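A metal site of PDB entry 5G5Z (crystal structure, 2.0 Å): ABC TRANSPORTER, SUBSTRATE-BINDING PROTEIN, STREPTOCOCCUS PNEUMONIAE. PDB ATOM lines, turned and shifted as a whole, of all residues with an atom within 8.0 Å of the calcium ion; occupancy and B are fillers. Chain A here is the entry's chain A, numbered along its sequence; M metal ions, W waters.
N of Asp 219 sits at hydrogen-bond distance from O of Val 211 (2.8 Å).
The nearest printed residue that does not touch the calcium ion is Thr 221 (4.6 Å).
Water W3 is bound to the calcium ion, 2.3 Å away. OD1 of Asn 224 is bound to the calcium ion (2.3 Å). The calcium ion is bound by water W2, at 2.4 Å. OD1 of Asp 219 binds the calcium ion (2.4 Å). The side-chain carboxylate (OD1) of Asp 223 is bound to the calcium ion. O of Phe 220 is bound to the calcium ion, at 2.5 Å. Water W1 is bound to the calcium ion (2.5 Å).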
ATOM      1  N   ILE A 203      15.422 -12.397  -3.645  1.00  0.00           N
ATOM      2  CA  ILE A 203      14.348 -11.704  -2.946  1.00  0.00           C
ATOM      3  C   ILE A 203      14.423 -10.187  -3.131  1.00  0.00           C
ATOM      4  O   ILE A 203      13.464  -9.557  -3.564  1.00  0.00           O
ATOM      5  CB  ILE A 203      14.330 -12.071  -1.454  1.00  0.00           C
ATOM      6  CG1 ILE A 203      14.344 -13.596  -1.286  1.00  0.00           C
ATOM      7  CG2 ILE A 203      13.109 -11.455  -0.806  1.00  0.00           C
ATOM      8  CD1 ILE A 203      14.383 -14.054   0.165  1.00  0.00           C
ATOM      9  N   HIS A 209       9.966  -2.517   2.186  1.00  0.00           N
ATOM     10  CA  HIS A 209      10.693  -3.642   2.747  1.00  0.00           C
ATOM     11  C   HIS A 209       9.779  -4.863   2.919  1.00  0.00           C
ATOM     12  O   HIS A 209       9.907  -5.633   3.865  1.00  0.00           O
ATOM     13  CB  HIS A 209      11.349  -3.279   4.089  1.00  0.00           C
ATOM     14  CG  HIS A 209      12.084  -1.983   4.044  1.00  0.00           C
ATOM     15  ND1 HIS A 209      13.185  -1.777   3.234  1.00  0.00           N
ATOM     16  CD2 HIS A 209      11.877  -0.815   4.699  1.00  0.00           C
ATOM     17  CE1 HIS A 209      13.621  -0.534   3.396  1.00  0.00           C
ATOM     18  NE2 HIS A 209      12.845   0.067   4.283  1.00  0.00           N
ATOM     19  N   LEU A 210       8.828  -5.033   1.987  1.00  0.00           N
ATOM     20  CA  LEU A 210       7.830  -6.098   2.110  1.00  0.00           C
ATOM     21  C   LEU A 210       7.495  -6.682   0.739  1.00  0.00           C
ATOM     22  O   LEU A 210       7.081  -5.945  -0.170  1.00  0.00           O
ATOM     23  CB  LEU A 210       6.576  -5.567   2.798  1.00  0.00           C
ATOM     24  CG  LEU A 210       5.706  -6.665   3.414  1.00  0.00           C
ATOM     25  CD1 LEU A 210       6.255  -7.068   4.784  1.00  0.00           C
ATOM     26  CD2 LEU A 210       4.262  -6.214   3.496  1.00  0.00           C
ATOM     27  N   VAL A 211       7.721  -7.984   0.581  1.00  0.00           N
ATOM     28  CA  VAL A 211       7.317  -8.728  -0.604  1.00  0.00           C
ATOM     29  C   VAL A 211       6.377  -9.862  -0.173  1.00  0.00           C
ATOM     30  O   VAL A 211       6.240 -10.161   1.019  1.00  0.00           O
ATOM     31  CB  VAL A 211       8.506  -9.288  -1.391  1.00  0.00           C
ATOM     32  CG1 VAL A 211       9.425  -8.156  -1.896  1.00  0.00           C
ATOM     33  CG2 VAL A 211       9.278 -10.340  -0.576  1.00  0.00           C
ATOM     34  N   VAL A 218       3.835 -13.083   3.836  1.00  0.00           N
ATOM     35  CA  VAL A 218       4.494 -11.800   3.653  1.00  0.00           C
ATOM     36  C   VAL A 218       5.900 -11.917   4.211  1.00  0.00           C
ATOM     37  O   VAL A 218       6.150 -12.613   5.213  1.00  0.00           O
ATOM     38  CB  VAL A 218       3.702 -10.651   4.316  1.00  0.00           C
ATOM     39  CG1 VAL A 218       2.279 -10.614   3.801  1.00  0.00           C
ATOM     40  CG2 VAL A 218       3.721 -10.767   5.823  1.00  0.00           C
ATOM     41  N   ASP A 219       6.850 -11.306   3.518  1.00  0.00           N
ATOM     42  CA  ASP A 219       8.244 -11.415   3.896  1.00  0.00           C
ATOM     43  C   ASP A 219       8.795 -10.011   4.105  1.00  0.00           C
ATOM     44  O   ASP A 219       8.746  -9.194   3.189  1.00  0.00           O
ATOM     45  CB  ASP A 219       9.046 -12.126   2.807  1.00  0.00           C
ATOM     46  CG  ASP A 219      10.498 -12.306   3.200  1.00  0.00           C
ATOM     47  OD1 ASP A 219      10.815 -12.155   4.405  1.00  0.00           O
ATOM     48  OD2 ASP A 219      11.324 -12.597   2.308  1.00  0.00           O
ATOM     49  N   PHE A 220       9.295  -9.741   5.308  1.00  0.00           N
ATOM     50  CA  PHE A 220      10.027  -8.514   5.577  1.00  0.00           C
ATOM     51  C   PHE A 220      11.434  -8.656   4.995  1.00  0.00           C
ATOM     52  O   PHE A 220      12.237  -9.478   5.454  1.00  0.00           O
ATOM     53  CB  PHE A 220      10.045  -8.251   7.071  1.00  0.00           C
ATOM     54  CG  PHE A 220      10.780  -7.017   7.455  1.00  0.00           C
ATOM     55  CD1 PHE A 220      10.227  -5.776   7.190  1.00  0.00           C
ATOM     56  CD2 PHE A 220      12.010  -7.099   8.076  1.00  0.00           C
ATOM     57  CE1 PHE A 220      10.908  -4.629   7.540  1.00  0.00           C
ATOM     58  CE2 PHE A 220      12.688  -5.961   8.425  1.00  0.00           C
ATOM     59  CZ  PHE A 220      12.134  -4.720   8.161  1.00  0.00           C
ATOM     60  N   THR A 221      11.724  -7.884   3.957  1.00  0.00           N
ATOM     61  CA  THR A 221      12.957  -8.113   3.212  1.00  0.00           C
ATOM     62  C   THR A 221      14.196  -7.717   4.005  1.00  0.00           C
ATOM     63  O   THR A 221      15.269  -8.296   3.795  1.00  0.00           O
ATOM     64  CB  THR A 221      12.910  -7.328   1.905  1.00  0.00           C
ATOM     65  OG1 THR A 221      12.691  -5.948   2.206  1.00  0.00           O
ATOM     66  CG2 THR A 221      11.760  -7.815   1.061  1.00  0.00           C
ATOM     67  N   ALA A 222      14.070  -6.739   4.893  1.00  0.00           N
ATOM     68  CA  ALA A 222      15.232  -6.082   5.494  1.00  0.00           C
ATOM     69  C   ALA A 222      15.874  -6.889   6.611  1.00  0.00           C
ATOM     70  O   ALA A 222      16.826  -6.405   7.231  1.00  0.00           O
ATOM     71  CB  ALA A 222      14.847  -4.695   5.996  1.00  0.00           C
ATOM     72  N   ASP A 223      15.369  -8.098   6.903  1.00  0.00           N
ATOM     73  CA  ASP A 223      16.039  -8.973   7.853  1.00  0.00           C
ATOM     74  C   ASP A 223      16.442 -10.300   7.188  1.00  0.00           C
ATOM     75  O   ASP A 223      16.704 -11.277   7.891  1.00  0.00           O
ATOM     76  CB  ASP A 223      15.159  -9.209   9.089  1.00  0.00           C
ATOM     77  CG  ASP A 223      13.979 -10.120   8.803  1.00  0.00           C
ATOM     78  OD1 ASP A 223      13.645 -10.361   7.612  1.00  0.00           O
ATOM     79  OD2 ASP A 223      13.350 -10.601   9.789  1.00  0.00           O
ATOM     80  N   ASN A 224      16.496 -10.348   5.863  1.00  0.00           N
ATOM     81  CA  ASN A 224      16.892 -11.556   5.147  1.00  0.00           C
ATOM     82  C   ASN A 224      18.407 -11.660   4.990  1.00  0.00           C
ATOM     83  O   ASN A 224      19.112 -10.655   4.839  1.00  0.00           O
ATOM     84  CB  ASN A 224      16.250 -11.596   3.766  1.00  0.00           C
ATOM     85  CG  ASN A 224      14.774 -11.745   3.838  1.00  0.00           C
ATOM     86  OD1 ASN A 224      14.256 -12.116   4.885  1.00  0.00           O
ATOM     87  ND2 ASN A 224      14.083 -11.461   2.746  1.00  0.00           N
ATOM     88  N   ASP A 225      18.901 -12.916   4.977  1.00  0.00           N
ATOM     89  CA  ASP A 225      20.303 -13.125   4.609  1.00  0.00           C
ATOM     90  C   ASP A 225      20.624 -12.544   3.243  1.00  0.00           C
ATOM     91  O   ASP A 225      21.727 -12.038   3.020  1.00  0.00           O
ATOM     92  CB  ASP A 225      20.647 -14.618   4.631  1.00  0.00           C
ATOM     93  CG  ASP A 225      20.503 -15.225   6.012  1.00  0.00           C
ATOM     94  OD1 ASP A 225      20.593 -14.468   6.987  1.00  0.00           O
ATOM     95  OD2 ASP A 225      20.282 -16.449   6.104  1.00  0.00           O
ATOM     96  N   ASN A 226      19.655 -12.626   2.321  1.00  0.00           N
ATOM     97  CA  ASN A 226      19.832 -12.030   1.001  1.00  0.00           C
ATOM     98  C   ASN A 226      20.095 -10.540   1.103  1.00  0.00           C
ATOM     99  O   ASN A 226      20.912  -9.990   0.353  1.00  0.00           O
ATOM    100  CB  ASN A 226      18.568 -12.302   0.197  1.00  0.00           C
ATOM    101  CG  ASN A 226      18.145 -13.754   0.275  1.00  0.00           C
ATOM    102  OD1 ASN A 226      17.526 -14.185   1.254  1.00  0.00           O
ATOM    103  ND2 ASN A 226      18.494 -14.518  -0.746  1.00  0.00           N
ATOM    104  N   TYR A 227      19.374  -9.862   1.995  1.00  0.00           N
ATOM    105  CA  TYR A 227      19.534  -8.424   2.184  1.00  0.00           C
ATOM    106  C   TYR A 227      20.925  -8.115   2.726  1.00  0.00           C
ATOM    107  O   TYR A 227      21.598  -7.197   2.245  1.00  0.00           O
ATOM    108  CB  TYR A 227      18.430  -7.948   3.140  1.00  0.00           C
ATOM    109  CG  TYR A 227      18.377  -6.454   3.438  1.00  0.00           C
ATOM    110  CD1 TYR A 227      19.139  -5.918   4.455  1.00  0.00           C
ATOM    111  CD2 TYR A 227      17.519  -5.618   2.744  1.00  0.00           C
ATOM    112  CE1 TYR A 227      19.082  -4.570   4.755  1.00  0.00           C
ATOM    113  CE2 TYR A 227      17.443  -4.264   3.034  1.00  0.00           C
ATOM    114  CZ  TYR A 227      18.237  -3.748   4.035  1.00  0.00           C
ATOM    115  OH  TYR A 227      18.188  -2.393   4.357  1.00  0.00           O
ATOM    116  N   TRP A 463      24.700  -7.803  12.611  1.00  0.00           N
ATOM    117  CA  TRP A 463      23.452  -8.285  12.018  1.00  0.00           C
ATOM    118  C   TRP A 463      22.544  -8.928  13.065  1.00  0.00           C
ATOM    119  O   TRP A 463      21.328  -8.677  13.077  1.00  0.00           O
ATOM    120  CB  TRP A 463      23.785  -9.251  10.891  1.00  0.00           C
ATOM    121  CG  TRP A 463      22.617  -9.840  10.160  1.00  0.00           C
ATOM    122  CD1 TRP A 463      22.167 -11.126  10.239  1.00  0.00           C
ATOM    123  CD2 TRP A 463      21.776  -9.172   9.193  1.00  0.00           C
ATOM    124  NE1 TRP A 463      21.090 -11.299   9.399  1.00  0.00           N
ATOM    125  CE2 TRP A 463      20.829 -10.114   8.751  1.00  0.00           C
ATOM    126  CE3 TRP A 463      21.729  -7.881   8.669  1.00  0.00           C
ATOM    127  CZ2 TRP A 463      19.845  -9.800   7.807  1.00  0.00           C
ATOM    128  CZ3 TRP A 463      20.751  -7.568   7.733  1.00  0.00           C
ATOM    129  CH2 TRP A 463      19.826  -8.529   7.308  1.00  0.00           C
ATOM    130  N   LYS A 467      18.799  -7.631  14.158  1.00  0.00           N
ATOM    131  CA  LYS A 467      17.541  -8.365  14.116  1.00  0.00           C
ATOM    132  C   LYS A 467      16.844  -8.369  15.471  1.00  0.00           C
ATOM    133  O   LYS A 467      15.613  -8.251  15.547  1.00  0.00           O
ATOM    134  CB  LYS A 467      17.785  -9.791  13.619  1.00  0.00           C
ATOM    135  CG  LYS A 467      18.341  -9.824  12.220  1.00  0.00           C
ATOM    136  CD  LYS A 467      18.095 -11.159  11.563  1.00  0.00           C
ATOM    137  CE  LYS A 467      19.166 -12.161  11.915  1.00  0.00           C
ATOM    138  NZ  LYS A 467      18.891 -13.433  11.231  1.00  0.00           N
ATOM    139  N   LEU A 475       8.636  -6.214  15.068  1.00  0.00           N
ATOM    140  CA  LEU A 475       8.530  -6.694  13.695  1.00  0.00           C
ATOM    141  C   LEU A 475       7.584  -7.896  13.578  1.00  0.00           C
ATOM    142  O   LEU A 475       6.816  -8.000  12.617  1.00  0.00           O
ATOM    143  CB  LEU A 475       9.922  -7.043  13.171  1.00  0.00           C
ATOM    144  CG  LEU A 475      10.067  -7.656  11.781  1.00  0.00           C
ATOM    145  CD1 LEU A 475       9.428  -6.738  10.756  1.00  0.00           C
ATOM    146  CD2 LEU A 475      11.560  -7.948  11.425  1.00  0.00           C
ATOM    147  N   LEU A 479       4.424  -7.989  11.094  1.00  0.00           N
ATOM    148  CA  LEU A 479       4.169  -8.963  10.031  1.00  0.00           C
ATOM    149  C   LEU A 479       2.831  -9.666  10.222  1.00  0.00           C
ATOM    150  O   LEU A 479       2.080  -9.859   9.250  1.00  0.00           O
ATOM    151  CB  LEU A 479       5.304  -9.977   9.964  1.00  0.00           C
ATOM    152  CG  LEU A 479       6.566  -9.427   9.318  1.00  0.00           C
ATOM    153  CD1 LEU A 479       7.715 -10.398   9.494  1.00  0.00           C
ATOM    154  CD2 LEU A 479       6.274  -9.191   7.854  1.00  0.00           C
HETATM  155 CA    CA M   1      12.367 -11.834   6.205  1.00  0.00          CA
HETATM  156  O   HOH W   1      12.240 -14.366   5.979  1.00  0.00           O
HETATM  157  O   HOH W   2      10.208 -11.759   7.160  1.00  0.00           O
HETATM  158  O   HOH W   3      13.134 -13.097   7.985  1.00  0.00           O
